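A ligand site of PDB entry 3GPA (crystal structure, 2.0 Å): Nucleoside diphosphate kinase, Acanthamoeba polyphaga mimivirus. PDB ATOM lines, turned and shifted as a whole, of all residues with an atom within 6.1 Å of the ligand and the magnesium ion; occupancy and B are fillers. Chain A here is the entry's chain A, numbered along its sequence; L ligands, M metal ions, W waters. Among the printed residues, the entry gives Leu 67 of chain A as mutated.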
ATOM      1  N   LYS A  14      30.592 -26.104   1.275  1.00  0.00           N
ATOM      2  CA  LYS A  14      29.411 -26.644   1.956  1.00  0.00           C
ATOM      3  C   LYS A  14      29.761 -27.163   3.359  1.00  0.00           C
ATOM      4  O   LYS A  14      30.948 -27.333   3.680  1.00  0.00           O
ATOM      5  CB  LYS A  14      28.752 -27.714   1.087  1.00  0.00           C
ATOM      6  CG  LYS A  14      28.467 -27.246  -0.365  1.00  0.00           C
ATOM      7  CD  LYS A  14      27.656 -28.295  -1.143  1.00  0.00           C
ATOM      8  CE  LYS A  14      27.200 -27.773  -2.520  1.00  0.00           C
ATOM      9  NZ  LYS A  14      26.559 -28.851  -3.349  1.00  0.00           N
ATOM     10  N   TYR A  55      19.391 -22.071  -4.405  1.00  0.00           N
ATOM     11  CA  TYR A  55      19.035 -23.272  -5.132  1.00  0.00           C
ATOM     12  C   TYR A  55      17.603 -23.191  -5.669  1.00  0.00           C
ATOM     13  O   TYR A  55      16.923 -24.210  -5.798  1.00  0.00           O
ATOM     14  CB  TYR A  55      19.194 -24.502  -4.232  1.00  0.00           C
ATOM     15  CG  TYR A  55      20.628 -24.992  -4.100  1.00  0.00           C
ATOM     16  CD1 TYR A  55      21.256 -25.061  -2.851  1.00  0.00           C
ATOM     17  CD2 TYR A  55      21.358 -25.391  -5.211  1.00  0.00           C
ATOM     18  CE1 TYR A  55      22.569 -25.522  -2.722  1.00  0.00           C
ATOM     19  CE2 TYR A  55      22.663 -25.849  -5.093  1.00  0.00           C
ATOM     20  CZ  TYR A  55      23.270 -25.910  -3.853  1.00  0.00           C
ATOM     21  OH  TYR A  55      24.587 -26.371  -3.754  1.00  0.00           O
ATOM     22  N   HIS A  58      16.028 -25.522  -8.177  1.00  0.00           N
ATOM     23  CA  HIS A  58      15.869 -26.904  -7.754  1.00  0.00           C
ATOM     24  C   HIS A  58      14.607 -27.074  -6.900  1.00  0.00           C
ATOM     25  O   HIS A  58      14.381 -28.153  -6.355  1.00  0.00           O
ATOM     26  CB  HIS A  58      17.093 -27.352  -6.957  1.00  0.00           C
ATOM     27  CG  HIS A  58      18.372 -27.299  -7.736  1.00  0.00           C
ATOM     28  ND1 HIS A  58      18.971 -28.433  -8.256  1.00  0.00           N
ATOM     29  CD2 HIS A  58      19.170 -26.267  -8.086  1.00  0.00           C
ATOM     30  CE1 HIS A  58      20.079 -28.102  -8.893  1.00  0.00           C
ATOM     31  NE2 HIS A  58      20.234 -26.786  -8.798  1.00  0.00           N
ATOM     32  N   SER A  62      12.739 -33.556  -5.795  1.00  0.00           N
ATOM     33  CA  SER A  62      12.561 -34.372  -4.595  1.00  0.00           C
ATOM     34  C   SER A  62      13.564 -34.036  -3.500  1.00  0.00           C
ATOM     35  O   SER A  62      13.236 -34.069  -2.306  1.00  0.00           O
ATOM     36  CB  SER A  62      12.647 -35.856  -4.945  1.00  0.00           C
ATOM     37  OG  SER A  62      13.688 -36.087  -5.883  1.00  0.00           O
ATOM     38  N   TYR A  63      14.791 -33.688  -3.893  1.00  0.00           N
ATOM     39  CA  TYR A  63      15.872 -33.497  -2.945  1.00  0.00           C
ATOM     40  C   TYR A  63      15.923 -32.088  -2.354  1.00  0.00           C
ATOM     41  O   TYR A  63      16.760 -31.817  -1.496  1.00  0.00           O
ATOM     42  CB  TYR A  63      17.224 -33.834  -3.582  1.00  0.00           C
ATOM     43  CG  TYR A  63      17.533 -33.029  -4.829  1.00  0.00           C
ATOM     44  CD1 TYR A  63      18.105 -31.767  -4.744  1.00  0.00           C
ATOM     45  CD2 TYR A  63      17.247 -33.540  -6.091  1.00  0.00           C
ATOM     46  CE1 TYR A  63      18.365 -31.024  -5.886  1.00  0.00           C
ATOM     47  CE2 TYR A  63      17.513 -32.819  -7.231  1.00  0.00           C
ATOM     48  CZ  TYR A  63      18.072 -31.554  -7.128  1.00  0.00           C
ATOM     49  OH  TYR A  63      18.330 -30.835  -8.263  1.00  0.00           O
ATOM     50  N   ASP A  66      15.765 -31.696   1.594  1.00  0.00           N
ATOM     51  CA  ASP A  66      16.896 -32.331   2.256  1.00  0.00           C
ATOM     52  C   ASP A  66      18.180 -31.547   2.006  1.00  0.00           C
ATOM     53  O   ASP A  66      19.004 -31.380   2.901  1.00  0.00           O
ATOM     54  CB  ASP A  66      17.037 -33.788   1.798  1.00  0.00           C
ATOM     55  CG  ASP A  66      15.921 -34.674   2.323  1.00  0.00           C
ATOM     56  OD1 ASP A  66      15.545 -34.512   3.509  1.00  0.00           O
ATOM     57  OD2 ASP A  66      15.422 -35.529   1.570  1.00  0.00           O
ATOM     58  N   LEU A  67      18.346 -31.072   0.772  1.00  0.00           N
ATOM     59  CA  LEU A  67      19.465 -30.209   0.419  1.00  0.00           C
ATOM     60  C   LEU A  67      19.523 -28.939   1.274  1.00  0.00           C
ATOM     61  O   LEU A  67      20.570 -28.594   1.820  1.00  0.00           O
ATOM     62  CB  LEU A  67      19.364 -29.812  -1.058  1.00  0.00           C
ATOM     63  CG  LEU A  67      20.330 -28.746  -1.581  1.00  0.00           C
ATOM     64  CD1 LEU A  67      21.781 -29.179  -1.408  1.00  0.00           C
ATOM     65  CD2 LEU A  67      20.035 -28.456  -3.049  1.00  0.00           C
ATOM     66  N   PHE A  70      20.558 -29.751   4.781  1.00  0.00           N
ATOM     67  CA  PHE A  70      22.000 -29.993   4.843  1.00  0.00           C
ATOM     68  C   PHE A  70      22.788 -28.678   4.812  1.00  0.00           C
ATOM     69  O   PHE A  70      23.723 -28.475   5.576  1.00  0.00           O
ATOM     70  CB  PHE A  70      22.406 -30.917   3.694  1.00  0.00           C
ATOM     71  CG  PHE A  70      23.874 -30.893   3.383  1.00  0.00           C
ATOM     72  CD1 PHE A  70      24.327 -30.491   2.126  1.00  0.00           C
ATOM     73  CD2 PHE A  70      24.818 -31.289   4.328  1.00  0.00           C
ATOM     74  CE1 PHE A  70      25.685 -30.470   1.835  1.00  0.00           C
ATOM     75  CE2 PHE A  70      26.173 -31.274   4.030  1.00  0.00           C
ATOM     76  CZ  PHE A  70      26.599 -30.860   2.776  1.00  0.00           C
ATOM     77  N   MET A  71      22.403 -27.766   3.917  1.00  0.00           N
ATOM     78  CA  MET A  71      23.137 -26.525   3.751  1.00  0.00           C
ATOM     79  C   MET A  71      23.055 -25.606   4.969  1.00  0.00           C
ATOM     80  O   MET A  71      23.873 -24.702   5.135  1.00  0.00           O
ATOM     81  CB  MET A  71      22.678 -25.797   2.486  1.00  0.00           C
ATOM     82  CG  MET A  71      23.015 -26.550   1.204  1.00  0.00           C
ATOM     83  SD  MET A  71      24.786 -26.605   0.840  1.00  0.00           S
ATOM     84  CE  MET A  71      25.092 -24.871   0.468  1.00  0.00           C
ATOM     85  N   ARG A  91      34.496 -24.531 -12.215  1.00  0.00           N
ATOM     86  CA  ARG A  91      33.533 -25.628 -12.397  1.00  0.00           C
ATOM     87  C   ARG A  91      34.236 -26.955 -12.672  1.00  0.00           C
ATOM     88  O   ARG A  91      33.874 -27.994 -12.115  1.00  0.00           O
ATOM     89  CB  ARG A  91      32.597 -25.322 -13.551  1.00  0.00           C
ATOM     90  CG  ARG A  91      31.173 -25.105 -13.140  1.00  0.00           C
ATOM     91  CD  ARG A  91      30.391 -26.400 -13.199  1.00  0.00           C
ATOM     92  NE  ARG A  91      29.511 -26.499 -12.048  1.00  0.00           N
ATOM     93  CZ  ARG A  91      28.455 -27.293 -11.953  1.00  0.00           C
ATOM     94  NH1 ARG A  91      28.093 -28.074 -12.965  1.00  0.00           N
ATOM     95  NH2 ARG A  91      27.756 -27.287 -10.830  1.00  0.00           N
ATOM     96  N   GLN A  94      35.822 -28.219  -9.633  1.00  0.00           N
ATOM     97  CA  GLN A  94      34.800 -28.851  -8.794  1.00  0.00           C
ATOM     98  C   GLN A  94      34.580 -30.291  -9.228  1.00  0.00           C
ATOM     99  O   GLN A  94      34.609 -31.215  -8.399  1.00  0.00           O
ATOM    100  CB  GLN A  94      33.473 -28.098  -8.905  1.00  0.00           C
ATOM    101  CG  GLN A  94      32.271 -28.916  -8.446  1.00  0.00           C
ATOM    102  CD  GLN A  94      30.952 -28.333  -8.896  1.00  0.00           C
ATOM    103  OE1 GLN A  94      30.461 -27.364  -8.327  1.00  0.00           O
ATOM    104  NE2 GLN A  94      30.361 -28.928  -9.927  1.00  0.00           N
ATOM    105  N   GLY A  95      34.351 -30.479 -10.519  1.00  0.00           N
ATOM    106  CA  GLY A  95      34.205 -31.810 -11.096  1.00  0.00           C
ATOM    107  C   GLY A  95      33.038 -32.583 -10.539  1.00  0.00           C
ATOM    108  O   GLY A  95      31.997 -32.019 -10.184  1.00  0.00           O
ATOM    109  N   ARG A 104      35.723 -32.830  -6.150  1.00  0.00           N
ATOM    110  CA  ARG A 104      34.753 -33.858  -5.796  1.00  0.00           C
ATOM    111  C   ARG A 104      35.260 -35.268  -6.109  1.00  0.00           C
ATOM    112  O   ARG A 104      34.975 -36.211  -5.378  1.00  0.00           O
ATOM    113  CB  ARG A 104      33.437 -33.633  -6.528  1.00  0.00           C
ATOM    114  CG  ARG A 104      32.608 -32.491  -5.977  1.00  0.00           C
ATOM    115  CD  ARG A 104      31.303 -32.393  -6.750  1.00  0.00           C
ATOM    116  NE  ARG A 104      30.543 -31.202  -6.403  1.00  0.00           N
ATOM    117  CZ  ARG A 104      29.398 -30.863  -6.983  1.00  0.00           C
ATOM    118  NH1 ARG A 104      28.880 -31.638  -7.931  1.00  0.00           N
ATOM    119  NH2 ARG A 104      28.774 -29.759  -6.593  1.00  0.00           N
ATOM    120  N   ILE A 111      25.830 -37.907  -3.321  1.00  0.00           N
ATOM    121  CA  ILE A 111      25.048 -37.049  -4.213  1.00  0.00           C
ATOM    122  C   ILE A 111      24.650 -35.722  -3.596  1.00  0.00           C
ATOM    123  O   ILE A 111      24.322 -34.789  -4.316  1.00  0.00           O
ATOM    124  CB  ILE A 111      23.731 -37.735  -4.699  1.00  0.00           C
ATOM    125  CG1 ILE A 111      23.178 -38.655  -3.620  1.00  0.00           C
ATOM    126  CG2 ILE A 111      23.943 -38.460  -6.007  1.00  0.00           C
ATOM    127  CD1 ILE A 111      22.280 -37.935  -2.629  1.00  0.00           C
ATOM    128  N   ARG A 112      24.656 -35.643  -2.265  1.00  0.00           N
ATOM    129  CA  ARG A 112      24.249 -34.414  -1.604  1.00  0.00           C
ATOM    130  C   ARG A 112      25.456 -33.726  -0.991  1.00  0.00           C
ATOM    131  O   ARG A 112      25.703 -32.560  -1.270  1.00  0.00           O
ATOM    132  CB  ARG A 112      23.225 -34.726  -0.509  1.00  0.00           C
ATOM    133  CG  ARG A 112      22.747 -33.531   0.288  1.00  0.00           C
ATOM    134  CD  ARG A 112      21.393 -33.845   0.916  1.00  0.00           C
ATOM    135  NE  ARG A 112      20.502 -34.339  -0.121  1.00  0.00           N
ATOM    136  CZ  ARG A 112      19.608 -35.306   0.044  1.00  0.00           C
ATOM    137  NH1 ARG A 112      19.481 -35.885   1.231  1.00  0.00           N
ATOM    138  NH2 ARG A 112      18.859 -35.709  -0.977  1.00  0.00           N
ATOM    139  N   GLU A 113      26.190 -34.470  -0.167  1.00  0.00           N
ATOM    140  CA  GLU A 113      27.346 -33.933   0.554  1.00  0.00           C
ATOM    141  C   GLU A 113      28.554 -34.019  -0.367  1.00  0.00           C
ATOM    142  O   GLU A 113      29.277 -35.031  -0.395  1.00  0.00           O
ATOM    143  CB  GLU A 113      27.541 -34.683   1.880  1.00  0.00           C
ATOM    144  CG  GLU A 113      26.277 -34.628   2.730  1.00  0.00           C
ATOM    145  CD  GLU A 113      26.468 -35.017   4.195  1.00  0.00           C
ATOM    146  OE1 GLU A 113      27.623 -35.189   4.647  1.00  0.00           O
ATOM    147  OE2 GLU A 113      25.447 -35.143   4.911  1.00  0.00           O
ATOM    148  N   ASN A 114      28.742 -32.970  -1.149  1.00  0.00           N
ATOM    149  CA  ASN A 114      29.809 -32.956  -2.133  1.00  0.00           C
ATOM    150  C   ASN A 114      30.709 -31.721  -2.032  1.00  0.00           C
ATOM    151  O   ASN A 114      31.289 -31.290  -3.031  1.00  0.00           O
ATOM    152  CB  ASN A 114      29.242 -33.174  -3.542  1.00  0.00           C
ATOM    153  CG  ASN A 114      28.211 -32.133  -3.921  1.00  0.00           C
ATOM    154  OD1 ASN A 114      28.175 -31.042  -3.357  1.00  0.00           O
ATOM    155  ND2 ASN A 114      27.356 -32.472  -4.895  1.00  0.00           N
ATOM    156  N   ILE A 116      31.470 -28.683  -2.276  1.00  0.00           N
ATOM    157  CA  ILE A 116      31.612 -27.409  -2.966  1.00  0.00           C
ATOM    158  C   ILE A 116      30.551 -27.177  -4.021  1.00  0.00           C
ATOM    159  O   ILE A 116      30.199 -28.091  -4.762  1.00  0.00           O
ATOM    160  CB  ILE A 116      33.002 -27.287  -3.638  1.00  0.00           C
ATOM    161  CG1 ILE A 116      33.111 -26.014  -4.463  1.00  0.00           C
ATOM    162  CG2 ILE A 116      33.295 -28.545  -4.522  1.00  0.00           C
ATOM    163  CD1 ILE A 116      34.545 -25.704  -4.892  1.00  0.00           C
ATOM    164  N   HIS A 117      30.040 -25.955  -4.069  1.00  0.00           N
ATOM    165  CA  HIS A 117      29.269 -25.477  -5.201  1.00  0.00           C
ATOM    166  C   HIS A 117      30.061 -24.457  -5.984  1.00  0.00           C
ATOM    167  O   HIS A 117      30.776 -23.630  -5.408  1.00  0.00           O
ATOM    168  CB  HIS A 117      27.969 -24.803  -4.756  1.00  0.00           C
ATOM    169  CG  HIS A 117      27.329 -23.963  -5.821  1.00  0.00           C
ATOM    170  ND1 HIS A 117      26.336 -24.432  -6.643  1.00  0.00           N
ATOM    171  CD2 HIS A 117      27.572 -22.693  -6.212  1.00  0.00           C
ATOM    172  CE1 HIS A 117      25.969 -23.481  -7.483  1.00  0.00           C
ATOM    173  NE2 HIS A 117      26.712 -22.409  -7.248  1.00  0.00           N
ATOM    174  N   ALA A 118      29.925 -24.495  -7.309  1.00  0.00           N
ATOM    175  CA  ALA A 118      30.503 -23.472  -8.165  1.00  0.00           C
ATOM    176  C   ALA A 118      29.481 -23.087  -9.240  1.00  0.00           C
ATOM    177  O   ALA A 118      28.773 -23.964  -9.751  1.00  0.00           O
ATOM    178  CB  ALA A 118      31.772 -23.992  -8.817  1.00  0.00           C
ATOM    179  N   ASP A 120      27.781 -22.248 -12.779  1.00  0.00           N
ATOM    180  CA  ASP A 120      27.971 -22.986 -14.036  1.00  0.00           C
ATOM    181  C   ASP A 120      27.784 -22.167 -15.311  1.00  0.00           C
ATOM    182  O   ASP A 120      27.937 -22.681 -16.411  1.00  0.00           O
ATOM    183  CB  ASP A 120      27.084 -24.241 -14.072  1.00  0.00           C
ATOM    184  CG  ASP A 120      25.616 -23.923 -14.253  1.00  0.00           C
ATOM    185  OD1 ASP A 120      25.261 -22.722 -14.297  1.00  0.00           O
ATOM    186  OD2 ASP A 120      24.809 -24.877 -14.383  1.00  0.00           O
HETATM  187  O1  LIG L   1      26.195 -29.072  -7.804  1.00  0.00           O
HETATM  188  P1  LIG L   1      26.024 -29.674  -9.177  1.00  0.00           P
HETATM  189  O2  LIG L   1      25.694 -28.694 -10.271  1.00  0.00           O
HETATM  190  O3  LIG L   1      27.102 -30.655  -9.573  1.00  0.00           O
HETATM  191  O4  LIG L   1      24.764 -30.665  -8.938  1.00  0.00           O
HETATM  192  P2  LIG L   1      23.212 -30.407  -9.291  1.00  0.00           P
HETATM  193  O5  LIG L   1      23.038 -29.272 -10.259  1.00  0.00           O
HETATM  194  O6  LIG L   1      22.541 -31.734  -9.537  1.00  0.00           O
HETATM  195  O7  LIG L   1      22.722 -29.749  -7.921  1.00  0.00           O
HETATM  196  C1  LIG L   1      22.205 -30.532  -6.889  1.00  0.00           C
HETATM  197  C2  LIG L   1      22.955 -30.047  -5.685  1.00  0.00           C
HETATM  198  O8  LIG L   1      22.065 -30.337  -4.624  1.00  0.00           O
HETATM  199  C3  LIG L   1      24.160 -30.962  -5.531  1.00  0.00           C
HETATM  200  O9  LIG L   1      25.416 -30.282  -5.554  1.00  0.00           O
HETATM  201  C4  LIG L   1      23.957 -31.693  -4.233  1.00  0.00           C
HETATM  202  O10 LIG L   1      24.583 -30.932  -3.190  1.00  0.00           O
HETATM  203  C5  LIG L   1      22.458 -31.563  -4.006  1.00  0.00           C
HETATM  204  N1  LIG L   1      21.707 -32.735  -4.476  1.00  0.00           N
HETATM  205  C6  LIG L   1      21.042 -33.441  -3.471  1.00  0.00           C
HETATM  206  O11 LIG L   1      21.130 -32.985  -2.312  1.00  0.00           O
HETATM  207  N2  LIG L   1      20.325 -34.546  -3.749  1.00  0.00           N
HETATM  208  C7  LIG L   1      20.247 -34.996  -5.031  1.00  0.00           C
HETATM  209  N3  LIG L   1      19.518 -36.112  -5.293  1.00  0.00           N
HETATM  210  C8  LIG L   1      20.917 -34.308  -6.051  1.00  0.00           C
HETATM  211  C9  LIG L   1      21.666 -33.180  -5.740  1.00  0.00           C
HETATM  212 MG    MG M   1      23.834 -27.615 -11.262  1.00  0.00          MG
HETATM  213  O   HOH W   1      25.304 -26.339 -12.169  1.00  0.00           O
HETATM  214  O   HOH W   2      20.128 -32.136 -10.023  1.00  0.00           O
HETATM  215  O   HOH W   3      28.558 -31.088 -11.671  1.00  0.00           O
HETATM  216  O   HOH W   4      25.867 -27.342  -5.861  1.00  0.00           O
HETATM  217  O   HOH W   5      24.009 -26.493  -9.129  1.00  0.00           O
HETATM  218  O   HOH W   6      23.122 -32.189 -12.313  1.00  0.00           O
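A nitrogen (N1) of the ligand lies close to the backbone carbonyl oxygen (O) of Ile 111, 3.3 Å away. Merely in contact with the ligand: His 58, Tyr 63, Leu 67 and Gln 94. Ten residues have an atom within 4 Å of the ligand: Lys 14, His 58, Tyr 63, Leu 67, Arg 91, Gln 94, Arg 104, Ile 111, Arg 112 and Asn 114. Along chain A the residues within 4 Å of the ligand span positions 14 to 114. The nearest printed residue that does not touch the ligand is Tyr 55 (4.2 Å).
NE2 of Gln 94 sits close to NH2 of Arg 91, 3.2 Å away. The side-chain hydroxyl (OH) of Tyr 63 sits at hydrogen-bond distance from a ring nitrogen (ND1) of His 58, at 2.5 Å. The guanidinium group (NH2) of Arg 104 sits at hydrogen-bond distance from the backbone carbonyl oxygen (O) of Ile 116, 2.9 Å away. The side-chain amide oxygen (OE1) of Gln 94 is in hydrogen-bond range of the backbone NH (N) of Ala 118, 3.1 Å away. NE of Arg 104 lies close to O of Asn 114 (3.5 Å). N of Arg 104 is in hydrogen-bond range of O of Gln 94 (3.0 Å). The backbone carbonyl oxygen (O) of Ala 118 sits at hydrogen-bond distance from the guanidinium group (NE) of Arg 91, 3.5 Å away. OH of Tyr 55 lies within hydrogen-bond range of NZ of Lys 14 (3.2 Å).
Water W1 lies within hydrogen-bond range of OD2 of Asp 120 (2.7 Å) and NH2 of Arg 91 (3.0 Å). Water W2 bridges O6 of the ligand (2.5 Å) and OH of Tyr 63 (2.8 Å). Water W3 lies within hydrogen-bond range of O3 of the ligand (2.6 Å), NE2 of Gln 94 (3.3 Å) and NH1 of Arg 91 (3.3 Å). Water W4 lies within hydrogen-bond range of an oxygen (O1) of the ligand, the side-chain hydroxyl (OH) of Tyr 55, the side-chain amino group (NZ) of Lys 14 and a ring nitrogen (ND1) of His 117.
Merely in contact with the magnesium ion: Arg 91 (3.96 Å). Of the 21 residues printed, 1 comes within 4 Å of the magnesium ion. The nearest printed residue that does not touch the magnesium ion is Asp 120 (4.3 Å).
The magnesium ion is bound by O5 of the ligand (2.1 Å). Water W1 is bound to the magnesium ion (2.1 Å). The magnesium ion is bound by O2 of the ligand, 2.4 Å away. Water W5 binds the magnesium ion, 2.4 Å away.
The guanidinium group (NE) of Arg 112 is in hydrogen-bond range of an oxygen (O11) of the ligand, 2.7 Å away. The guanidinium group of Arg 91 lies within salt-bridge range of an oxygen (O3) of the ligand, at 3.7 Å. O of Arg 112 is in hydrogen-bond range of O10 of the ligand (2.8 Å). ND2 of Asn 114 is in hydrogen-bond range of O9 of the ligand (3.0 Å). The side-chain amino group (NZ) of Lys 14 sits at hydrogen-bond distance from an oxygen (O9) of the ligand (2.9 Å). An oxygen (O3) of the ligand is in salt-bridge range of the guanidinium group (NH1) of Arg 104 (2.6 Å).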
